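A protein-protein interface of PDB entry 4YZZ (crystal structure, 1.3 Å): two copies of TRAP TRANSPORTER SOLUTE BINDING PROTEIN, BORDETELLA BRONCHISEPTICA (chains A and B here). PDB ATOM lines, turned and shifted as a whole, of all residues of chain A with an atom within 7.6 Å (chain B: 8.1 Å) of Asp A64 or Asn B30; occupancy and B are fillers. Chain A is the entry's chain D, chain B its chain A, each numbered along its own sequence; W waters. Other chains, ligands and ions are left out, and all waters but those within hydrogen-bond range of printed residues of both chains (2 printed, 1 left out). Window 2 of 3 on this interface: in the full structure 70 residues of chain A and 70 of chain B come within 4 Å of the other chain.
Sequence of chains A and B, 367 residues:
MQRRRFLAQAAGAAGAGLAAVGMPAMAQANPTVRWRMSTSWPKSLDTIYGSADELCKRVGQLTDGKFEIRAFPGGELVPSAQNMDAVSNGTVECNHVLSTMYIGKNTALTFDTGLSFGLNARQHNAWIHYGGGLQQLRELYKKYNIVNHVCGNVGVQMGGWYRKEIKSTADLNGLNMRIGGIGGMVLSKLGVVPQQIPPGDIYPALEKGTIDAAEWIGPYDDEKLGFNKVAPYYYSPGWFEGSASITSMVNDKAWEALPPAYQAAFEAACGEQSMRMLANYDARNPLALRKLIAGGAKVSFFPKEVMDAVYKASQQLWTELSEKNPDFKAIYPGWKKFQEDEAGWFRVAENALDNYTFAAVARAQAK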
ATOM      1  N   ASN A  30      10.404  25.435   2.344  1.00  0.00           N
ATOM      2  CA  ASN A  30      10.009  24.798   3.595  1.00  0.00           C
ATOM      3  C   ASN A  30       8.895  23.769   3.352  1.00  0.00           C
ATOM      4  O   ASN A  30       7.793  23.903   3.889  1.00  0.00           O
ATOM      5  CB  ASN A  30       9.556  25.879   4.589  1.00  0.00           C
ATOM      6  CG  ASN A  30       9.251  25.331   5.983  1.00  0.00           C
ATOM      7  OD1 ASN A  30       9.792  24.308   6.401  1.00  0.00           O
ATOM      8  ND2 ASN A  30       8.381  26.030   6.712  1.00  0.00           N
ATOM      9  N   PRO A  31       9.167  22.741   2.528  1.00  0.00           N
ATOM     10  CA  PRO A  31       8.124  21.731   2.348  1.00  0.00           C
ATOM     11  C   PRO A  31       7.936  20.890   3.596  1.00  0.00           C
ATOM     12  O   PRO A  31       8.825  20.797   4.435  1.00  0.00           O
ATOM     13  CB  PRO A  31       8.645  20.878   1.188  1.00  0.00           C
ATOM     14  CG  PRO A  31      10.124  21.052   1.219  1.00  0.00           C
ATOM     15  CD  PRO A  31      10.372  22.443   1.735  1.00  0.00           C
ATOM     16  N   ARG A  58       0.856  18.877  -9.999  1.00  0.00           N
ATOM     17  CA  ARG A  58      -0.475  18.851  -9.428  1.00  0.00           C
ATOM     18  C   ARG A  58      -0.414  18.569  -7.929  1.00  0.00           C
ATOM     19  O   ARG A  58      -1.112  19.199  -7.140  1.00  0.00           O
ATOM     20  CB  ARG A  58      -1.339  17.801 -10.123  1.00  0.00           C
ATOM     21  CG  ARG A  58      -2.719  17.632  -9.526  1.00  0.00           C
ATOM     22  CD  ARG A  58      -3.563  18.864  -9.722  1.00  0.00           C
ATOM     23  NE  ARG A  58      -4.348  18.801 -10.952  1.00  0.00           N
ATOM     24  CZ  ARG A  58      -4.966  19.827 -11.528  1.00  0.00           C
ATOM     25  NH1 ARG A  58      -4.784  21.055 -11.094  1.00  0.00           N
ATOM     26  NH2 ARG A  58      -5.734  19.605 -12.578  1.00  0.00           N
ATOM     27  N   VAL A  59       0.439  17.636  -7.521  1.00  0.00           N
ATOM     28  CA  VAL A  59       0.578  17.374  -6.091  1.00  0.00           C
ATOM     29  C   VAL A  59       1.033  18.641  -5.346  1.00  0.00           C
ATOM     30  O   VAL A  59       0.547  18.928  -4.260  1.00  0.00           O
ATOM     31  CB  VAL A  59       1.531  16.201  -5.831  1.00  0.00           C
ATOM     32  CG1 VAL A  59       1.900  16.071  -4.350  1.00  0.00           C
ATOM     33  CG2 VAL A  59       0.889  14.914  -6.322  1.00  0.00           C
ATOM     34  N   GLY A  60       1.944  19.405  -5.945  1.00  0.00           N
ATOM     35  CA  GLY A  60       2.331  20.688  -5.381  1.00  0.00           C
ATOM     36  C   GLY A  60       1.137  21.634  -5.277  1.00  0.00           C
ATOM     37  O   GLY A  60       0.927  22.268  -4.251  1.00  0.00           O
ATOM     38  N   GLN A  61       0.375  21.767  -6.346  1.00  0.00           N
ATOM     39  CA  GLN A  61      -0.777  22.657  -6.312  1.00  0.00           C
ATOM     40  C   GLN A  61      -1.751  22.284  -5.197  1.00  0.00           C
ATOM     41  O   GLN A  61      -2.284  23.134  -4.481  1.00  0.00           O
ATOM     42  CB  GLN A  61      -1.516  22.600  -7.642  1.00  0.00           C
ATOM     43  CG  GLN A  61      -0.793  23.264  -8.812  1.00  0.00           C
ATOM     44  CD  GLN A  61      -1.494  23.013 -10.120  1.00  0.00           C
ATOM     45  OE1 GLN A  61      -2.211  22.029 -10.259  1.00  0.00           O
ATOM     46  NE2 GLN A  61      -1.303  23.904 -11.086  1.00  0.00           N
ATOM     47  N   LEU A  62      -2.011  20.997  -5.091  1.00  0.00           N
ATOM     48  CA  LEU A  62      -2.959  20.487  -4.120  1.00  0.00           C
ATOM     49  C   LEU A  62      -2.535  20.753  -2.685  1.00  0.00           C
ATOM     50  O   LEU A  62      -3.359  20.792  -1.792  1.00  0.00           O
ATOM     51  CB  LEU A  62      -3.162  18.991  -4.321  1.00  0.00           C
ATOM     52  CG  LEU A  62      -3.899  18.612  -5.615  1.00  0.00           C
ATOM     53  CD1 LEU A  62      -3.811  17.112  -5.872  1.00  0.00           C
ATOM     54  CD2 LEU A  62      -5.357  19.052  -5.541  1.00  0.00           C
ATOM     55  N   THR A  63      -1.235  20.926  -2.474  1.00  0.00           N
ATOM     56  CA  THR A  63      -0.693  21.032  -1.125  1.00  0.00           C
ATOM     57  C   THR A  63       0.013  22.371  -0.895  1.00  0.00           C
ATOM     58  O   THR A  63       0.738  22.526   0.092  1.00  0.00           O
ATOM     59  CB  THR A  63       0.303  19.896  -0.836  1.00  0.00           C
ATOM     60  OG1 THR A  63       1.423  20.013  -1.726  1.00  0.00           O
ATOM     61  CG2 THR A  63      -0.358  18.544  -1.005  1.00  0.00           C
ATOM     62  N   ASP A  64      -0.217  23.359  -1.767  1.00  0.00           N
ATOM     63  CA  ASP A  64       0.445  24.667  -1.653  1.00  0.00           C
ATOM     64  C   ASP A  64       1.959  24.507  -1.584  1.00  0.00           C
ATOM     65  O   ASP A  64       2.640  25.233  -0.854  1.00  0.00           O
ATOM     66  CB  ASP A  64      -0.099  25.458  -0.453  1.00  0.00           C
ATOM     67  CG  ASP A  64      -1.540  25.886  -0.644  1.00  0.00           C
ATOM     68  OD1 ASP A  64      -1.834  26.460  -1.709  1.00  0.00           O
ATOM     69  OD2 ASP A  64      -2.359  25.659   0.266  1.00  0.00           O
ATOM     70  N   GLY A  65       2.480  23.549  -2.339  1.00  0.00           N
ATOM     71  CA  GLY A  65       3.904  23.319  -2.451  1.00  0.00           C
ATOM     72  C   GLY A  65       4.492  22.514  -1.325  1.00  0.00           C
ATOM     73  O   GLY A  65       5.689  22.205  -1.352  1.00  0.00           O
ATOM     74  N   LYS A  66       3.692  22.146  -0.341  1.00  0.00           N
ATOM     75  CA  LYS A  66       4.227  21.510   0.853  1.00  0.00           C
ATOM     76  C   LYS A  66       4.493  20.008   0.714  1.00  0.00           C
ATOM     77  O   LYS A  66       5.248  19.452   1.509  1.00  0.00           O
ATOM     78  CB  LYS A  66       3.324  21.818   2.042  1.00  0.00           C
ATOM     79  CG  LYS A  66       3.344  23.319   2.387  1.00  0.00           C
ATOM     80  CD  LYS A  66       3.078  23.617   3.851  1.00  0.00           C
ATOM     81  CE  LYS A  66       3.657  24.990   4.259  1.00  0.00           C
ATOM     82  NZ  LYS A  66       5.054  24.923   4.810  1.00  0.00           N
ATOM     83  N   PHE A  67       3.914  19.357  -0.290  1.00  0.00           N
ATOM     84  CA  PHE A  67       4.311  17.997  -0.676  1.00  0.00           C
ATOM     85  C   PHE A  67       5.042  18.177  -1.994  1.00  0.00           C
ATOM     86  O   PHE A  67       4.429  18.358  -3.043  1.00  0.00           O
ATOM     87  CB  PHE A  67       3.082  17.086  -0.806  1.00  0.00           C
ATOM     88  CG  PHE A  67       3.389  15.626  -1.082  1.00  0.00           C
ATOM     89  CD1 PHE A  67       4.692  15.125  -1.149  1.00  0.00           C
ATOM     90  CD2 PHE A  67       2.343  14.748  -1.303  1.00  0.00           C
ATOM     91  CE1 PHE A  67       4.915  13.792  -1.403  1.00  0.00           C
ATOM     92  CE2 PHE A  67       2.569  13.423  -1.571  1.00  0.00           C
ATOM     93  CZ  PHE A  67       3.854  12.938  -1.608  1.00  0.00           C
ATOM     94  N   TYR A 262      -2.171  14.051   1.783  1.00  0.00           N
ATOM     95  CA  TYR A 262      -1.089  13.887   0.817  1.00  0.00           C
ATOM     96  C   TYR A 262      -1.192  12.554   0.083  1.00  0.00           C
ATOM     97  O   TYR A 262      -0.895  12.489  -1.114  1.00  0.00           O
ATOM     98  CB  TYR A 262       0.266  13.998   1.498  1.00  0.00           C
ATOM     99  CG  TYR A 262       0.659  15.383   1.994  1.00  0.00           C
ATOM    100  CD1 TYR A 262      -0.257  16.425   2.087  1.00  0.00           C
ATOM    101  CD2 TYR A 262       1.973  15.630   2.364  1.00  0.00           C
ATOM    102  CE1 TYR A 262       0.136  17.682   2.556  1.00  0.00           C
ATOM    103  CE2 TYR A 262       2.373  16.878   2.837  1.00  0.00           C
ATOM    104  CZ  TYR A 262       1.446  17.885   2.926  1.00  0.00           C
ATOM    105  OH  TYR A 262       1.879  19.117   3.390  1.00  0.00           O
ATOM    106  N   ASN B  30      -5.782  27.455   4.615  1.00  0.00           N
ATOM    107  CA  ASN B  30      -6.950  27.664   3.768  1.00  0.00           C
ATOM    108  C   ASN B  30      -8.247  27.606   4.592  1.00  0.00           C
ATOM    109  O   ASN B  30      -8.320  26.864   5.569  1.00  0.00           O
ATOM    110  CB  ASN B  30      -6.988  26.600   2.661  1.00  0.00           C
ATOM    111  CG  ASN B  30      -5.891  26.786   1.610  1.00  0.00           C
ATOM    112  OD1 ASN B  30      -5.739  27.866   1.035  1.00  0.00           O
ATOM    113  ND2 ASN B  30      -5.123  25.723   1.358  1.00  0.00           N
ATOM    114  N   PRO B  31      -9.278  28.376   4.189  1.00  0.00           N
ATOM    115  CA  PRO B  31     -10.551  28.535   4.914  1.00  0.00           C
ATOM    116  C   PRO B  31     -11.548  27.385   4.733  1.00  0.00           C
ATOM    117  O   PRO B  31     -11.357  26.512   3.879  1.00  0.00           O
ATOM    118  CB  PRO B  31     -11.149  29.778   4.259  1.00  0.00           C
ATOM    119  CG  PRO B  31     -10.721  29.658   2.843  1.00  0.00           C
ATOM    120  CD  PRO B  31      -9.289  29.155   2.934  1.00  0.00           C
ATOM    121  N   THR B  32     -12.612  27.397   5.534  1.00  0.00           N
ATOM    122  CA  THR B  32     -13.691  26.432   5.392  1.00  0.00           C
ATOM    123  C   THR B  32     -14.620  26.950   4.323  1.00  0.00           C
ATOM    124  O   THR B  32     -15.032  28.105   4.361  1.00  0.00           O
ATOM    125  CB  THR B  32     -14.489  26.247   6.690  1.00  0.00           C
ATOM    126  OG1 THR B  32     -13.614  25.764   7.714  1.00  0.00           O
ATOM    127  CG2 THR B  32     -15.630  25.247   6.493  1.00  0.00           C
ATOM    128  N   VAL B  33     -14.929  26.083   3.368  1.00  0.00           N
ATOM    129  CA  VAL B  33     -15.823  26.414   2.265  1.00  0.00           C
ATOM    130  C   VAL B  33     -16.841  25.299   2.135  1.00  0.00           C
ATOM    131  O   VAL B  33     -16.479  24.120   2.133  1.00  0.00           O
ATOM    132  CB  VAL B  33     -15.023  26.557   0.957  1.00  0.00           C
ATOM    133  CG1 VAL B  33     -15.944  26.832  -0.229  1.00  0.00           C
ATOM    134  CG2 VAL B  33     -14.018  27.660   1.092  1.00  0.00           C
ATOM    135  N   LEU B  62      -8.735  15.789  -0.092  1.00  0.00           N
ATOM    136  CA  LEU B  62      -7.646  16.655  -0.529  1.00  0.00           C
ATOM    137  C   LEU B  62      -7.488  17.885   0.335  1.00  0.00           C
ATOM    138  O   LEU B  62      -6.409  18.470   0.407  1.00  0.00           O
ATOM    139  CB  LEU B  62      -7.860  17.081  -1.973  1.00  0.00           C
ATOM    140  CG  LEU B  62      -7.762  15.950  -2.992  1.00  0.00           C
ATOM    141  CD1 LEU B  62      -8.229  16.367  -4.359  1.00  0.00           C
ATOM    142  CD2 LEU B  62      -6.323  15.462  -3.055  1.00  0.00           C
ATOM    143  N   THR B  63      -8.574  18.293   0.970  1.00  0.00           N
ATOM    144  CA  THR B  63      -8.584  19.509   1.781  1.00  0.00           C
ATOM    145  C   THR B  63      -8.838  19.278   3.280  1.00  0.00           C
ATOM    146  O   THR B  63      -9.145  20.227   4.006  1.00  0.00           O
ATOM    147  CB  THR B  63      -9.654  20.475   1.260  1.00  0.00           C
ATOM    148  OG1 THR B  63     -10.954  19.891   1.421  1.00  0.00           O
ATOM    149  CG2 THR B  63      -9.412  20.831  -0.202  1.00  0.00           C
ATOM    150  N   LYS B  66     -12.041  20.619   4.714  1.00  0.00           N
ATOM    151  CA  LYS B  66     -12.266  22.065   4.729  1.00  0.00           C
ATOM    152  C   LYS B  66     -13.085  22.559   3.545  1.00  0.00           C
ATOM    153  O   LYS B  66     -13.822  23.537   3.651  1.00  0.00           O
ATOM    154  CB  LYS B  66     -10.934  22.817   4.771  1.00  0.00           C
ATOM    155  CG  LYS B  66     -10.098  22.563   6.030  1.00  0.00           C
ATOM    156  CD  LYS B  66      -8.936  23.560   6.149  1.00  0.00           C
ATOM    157  CE  LYS B  66      -7.916  23.480   5.001  1.00  0.00           C
ATOM    158  NZ  LYS B  66      -7.253  22.171   4.819  1.00  0.00           N
ATOM    159  N   PHE B  67     -12.951  21.893   2.406  1.00  0.00           N
ATOM    160  CA  PHE B  67     -13.760  22.201   1.221  1.00  0.00           C
ATOM    161  C   PHE B  67     -14.786  21.086   1.145  1.00  0.00           C
ATOM    162  O   PHE B  67     -14.509  19.981   0.674  1.00  0.00           O
ATOM    163  CB  PHE B  67     -12.881  22.266  -0.038  1.00  0.00           C
ATOM    164  CG  PHE B  67     -13.587  22.760  -1.288  1.00  0.00           C
ATOM    165  CD1 PHE B  67     -14.904  23.219  -1.273  1.00  0.00           C
ATOM    166  CD2 PHE B  67     -12.909  22.756  -2.490  1.00  0.00           C
ATOM    167  CE1 PHE B  67     -15.500  23.654  -2.448  1.00  0.00           C
ATOM    168  CE2 PHE B  67     -13.512  23.194  -3.669  1.00  0.00           C
ATOM    169  CZ  PHE B  67     -14.806  23.639  -3.636  1.00  0.00           C
ATOM    170  N   LEU B 258     -12.473  30.635  -4.476  1.00  0.00           N
ATOM    171  CA  LEU B 258     -11.640  29.554  -3.968  1.00  0.00           C
ATOM    172  C   LEU B 258     -10.160  29.903  -3.987  1.00  0.00           C
ATOM    173  O   LEU B 258      -9.666  30.486  -4.954  1.00  0.00           O
ATOM    174  CB  LEU B 258     -11.815  28.314  -4.832  1.00  0.00           C
ATOM    175  CG  LEU B 258     -13.170  27.608  -4.868  1.00  0.00           C
ATOM    176  CD1 LEU B 258     -13.104  26.433  -5.847  1.00  0.00           C
ATOM    177  CD2 LEU B 258     -13.605  27.150  -3.479  1.00  0.00           C
ATOM    178  N   PRO B 259      -9.428  29.464  -2.958  1.00  0.00           N
ATOM    179  CA  PRO B 259      -7.967  29.541  -3.004  1.00  0.00           C
ATOM    180  C   PRO B 259      -7.424  28.574  -4.047  1.00  0.00           C
ATOM    181  O   PRO B 259      -8.116  27.611  -4.431  1.00  0.00           O
ATOM    182  CB  PRO B 259      -7.533  29.142  -1.584  1.00  0.00           C
ATOM    183  CG  PRO B 259      -8.616  28.338  -1.062  1.00  0.00           C
ATOM    184  CD  PRO B 259      -9.905  28.803  -1.730  1.00  0.00           C
ATOM    185  N   PRO B 260      -6.199  28.815  -4.522  1.00  0.00           N
ATOM    186  CA  PRO B 260      -5.619  27.997  -5.592  1.00  0.00           C
ATOM    187  C   PRO B 260      -5.616  26.495  -5.288  1.00  0.00           C
ATOM    188  O   PRO B 260      -5.892  25.695  -6.189  1.00  0.00           O
ATOM    189  CB  PRO B 260      -4.190  28.532  -5.706  1.00  0.00           C
ATOM    190  CG  PRO B 260      -4.316  29.966  -5.307  1.00  0.00           C
ATOM    191  CD  PRO B 260      -5.366  29.999  -4.233  1.00  0.00           C
ATOM    192  N   ALA B 261      -5.331  26.100  -4.053  1.00  0.00           N
ATOM    193  CA  ALA B 261      -5.295  24.676  -3.739  1.00  0.00           C
ATOM    194  C   ALA B 261      -6.675  24.038  -3.873  1.00  0.00           C
ATOM    195  O   ALA B 261      -6.777  22.860  -4.234  1.00  0.00           O
ATOM    196  CB  ALA B 261      -4.751  24.441  -2.334  1.00  0.00           C
ATOM    197  N   TYR B 262      -7.740  24.808  -3.614  1.00  0.00           N
ATOM    198  CA  TYR B 262      -9.092  24.262  -3.687  1.00  0.00           C
ATOM    199  C   TYR B 262      -9.553  24.174  -5.141  1.00  0.00           C
ATOM    200  O   TYR B 262     -10.271  23.247  -5.510  1.00  0.00           O
ATOM    201  CB  TYR B 262     -10.090  25.087  -2.883  1.00  0.00           C
ATOM    202  CG  TYR B 262      -9.943  25.023  -1.382  1.00  0.00           C
ATOM    203  CD1 TYR B 262      -8.832  24.443  -0.778  1.00  0.00           C
ATOM    204  CD2 TYR B 262     -10.931  25.552  -0.558  1.00  0.00           C
ATOM    205  CE1 TYR B 262      -8.712  24.413   0.599  1.00  0.00           C
ATOM    206  CE2 TYR B 262     -10.822  25.531   0.814  1.00  0.00           C
ATOM    207  CZ  TYR B 262      -9.708  24.969   1.388  1.00  0.00           C
ATOM    208  OH  TYR B 262      -9.590  24.946   2.758  1.00  0.00           O
ATOM    209  N   ALA B 264      -7.419  23.578  -7.587  1.00  0.00           N
ATOM    210  CA  ALA B 264      -6.685  22.385  -7.981  1.00  0.00           C
ATOM    211  C   ALA B 264      -7.383  21.116  -7.496  1.00  0.00           C
ATOM    212  O   ALA B 264      -7.442  20.123  -8.236  1.00  0.00           O
ATOM    213  CB  ALA B 264      -5.235  22.442  -7.456  1.00  0.00           C
HETATM  214  O   HOH W   1      -4.220  27.664  -1.779  1.00  0.00           O
HETATM  215  O   HOH W   2      -3.787  17.710  -0.411  1.00  0.00           O
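The guanidinium group (NH1) of Arg A58 sits at hydrogen-bond distance from the side-chain amide oxygen (OE1) of Gln A61 (2.9 Å).
Asp A64 touches just these residues of chain B: Asn B30 (3.0 Å) and Ala B261 (3.6 Å).
Asn B30 touches one residue of chain A.
Of the printed residues of chain B, Arg A58 touches Ala B264.
Of the printed residues of chain B, Gln A61 touches Ala B261 (3.5 Å) and Ala B264 (3.7 Å).
Of the printed residues of chain A, Ala B261 touches Gln A61, Leu A62 and Asp A64.
The nearest residue of chain B that does not touch Asp A64 is Pro B260 (5.1 Å).
The nearest printed residue of chain A that does not touch Ala B264 is Thr A63 (6.6 Å).
Water W1 lies within hydrogen-bond range of the side-chain carboxylate (OD1) of Asp A64 (2.7 Å), the backbone NH (N) of Ala B261 (3.0 Å) and the side-chain amide oxygen (OD1) of Asn B30 (3.2 Å).
Water W2 bridges the backbone carbonyl oxygen (O) of Leu B62 (2.8 Å) and the backbone carbonyl oxygen (O) of Leu A62 (3.4 Å).
OD2 of Asp A64 lies within hydrogen-bond range of ND2 of Asn B30, 3.0 Å away.
Hydrophobic or aromatic side chains of chain B that line the printed part of chain A: Ala B261 and Ala B264.
Of the 13 printed residues of chain A, 4 touch a printed residue of chain B.
Hydrophobic or aromatic side chains of chain A that line the printed part of chain B: Leu A62.
Along chain A the printed residues that touch a printed residue of chain B span positions 58 to 64.
7 positions are printed for both chains.
Among the printed residues, pairs that only touch across the chains: Arg A58 with Ala B264 (3.9 Å), Gln A61 with Ala B261 (3.5 Å), Gln A61 with Ala B264 (3.7 Å), Leu A62 with Ala B261 (3.9 Å), Leu A62 with Ala B264 (3.5 Å) and Asp A64 with Ala B261 (3.6 Å).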
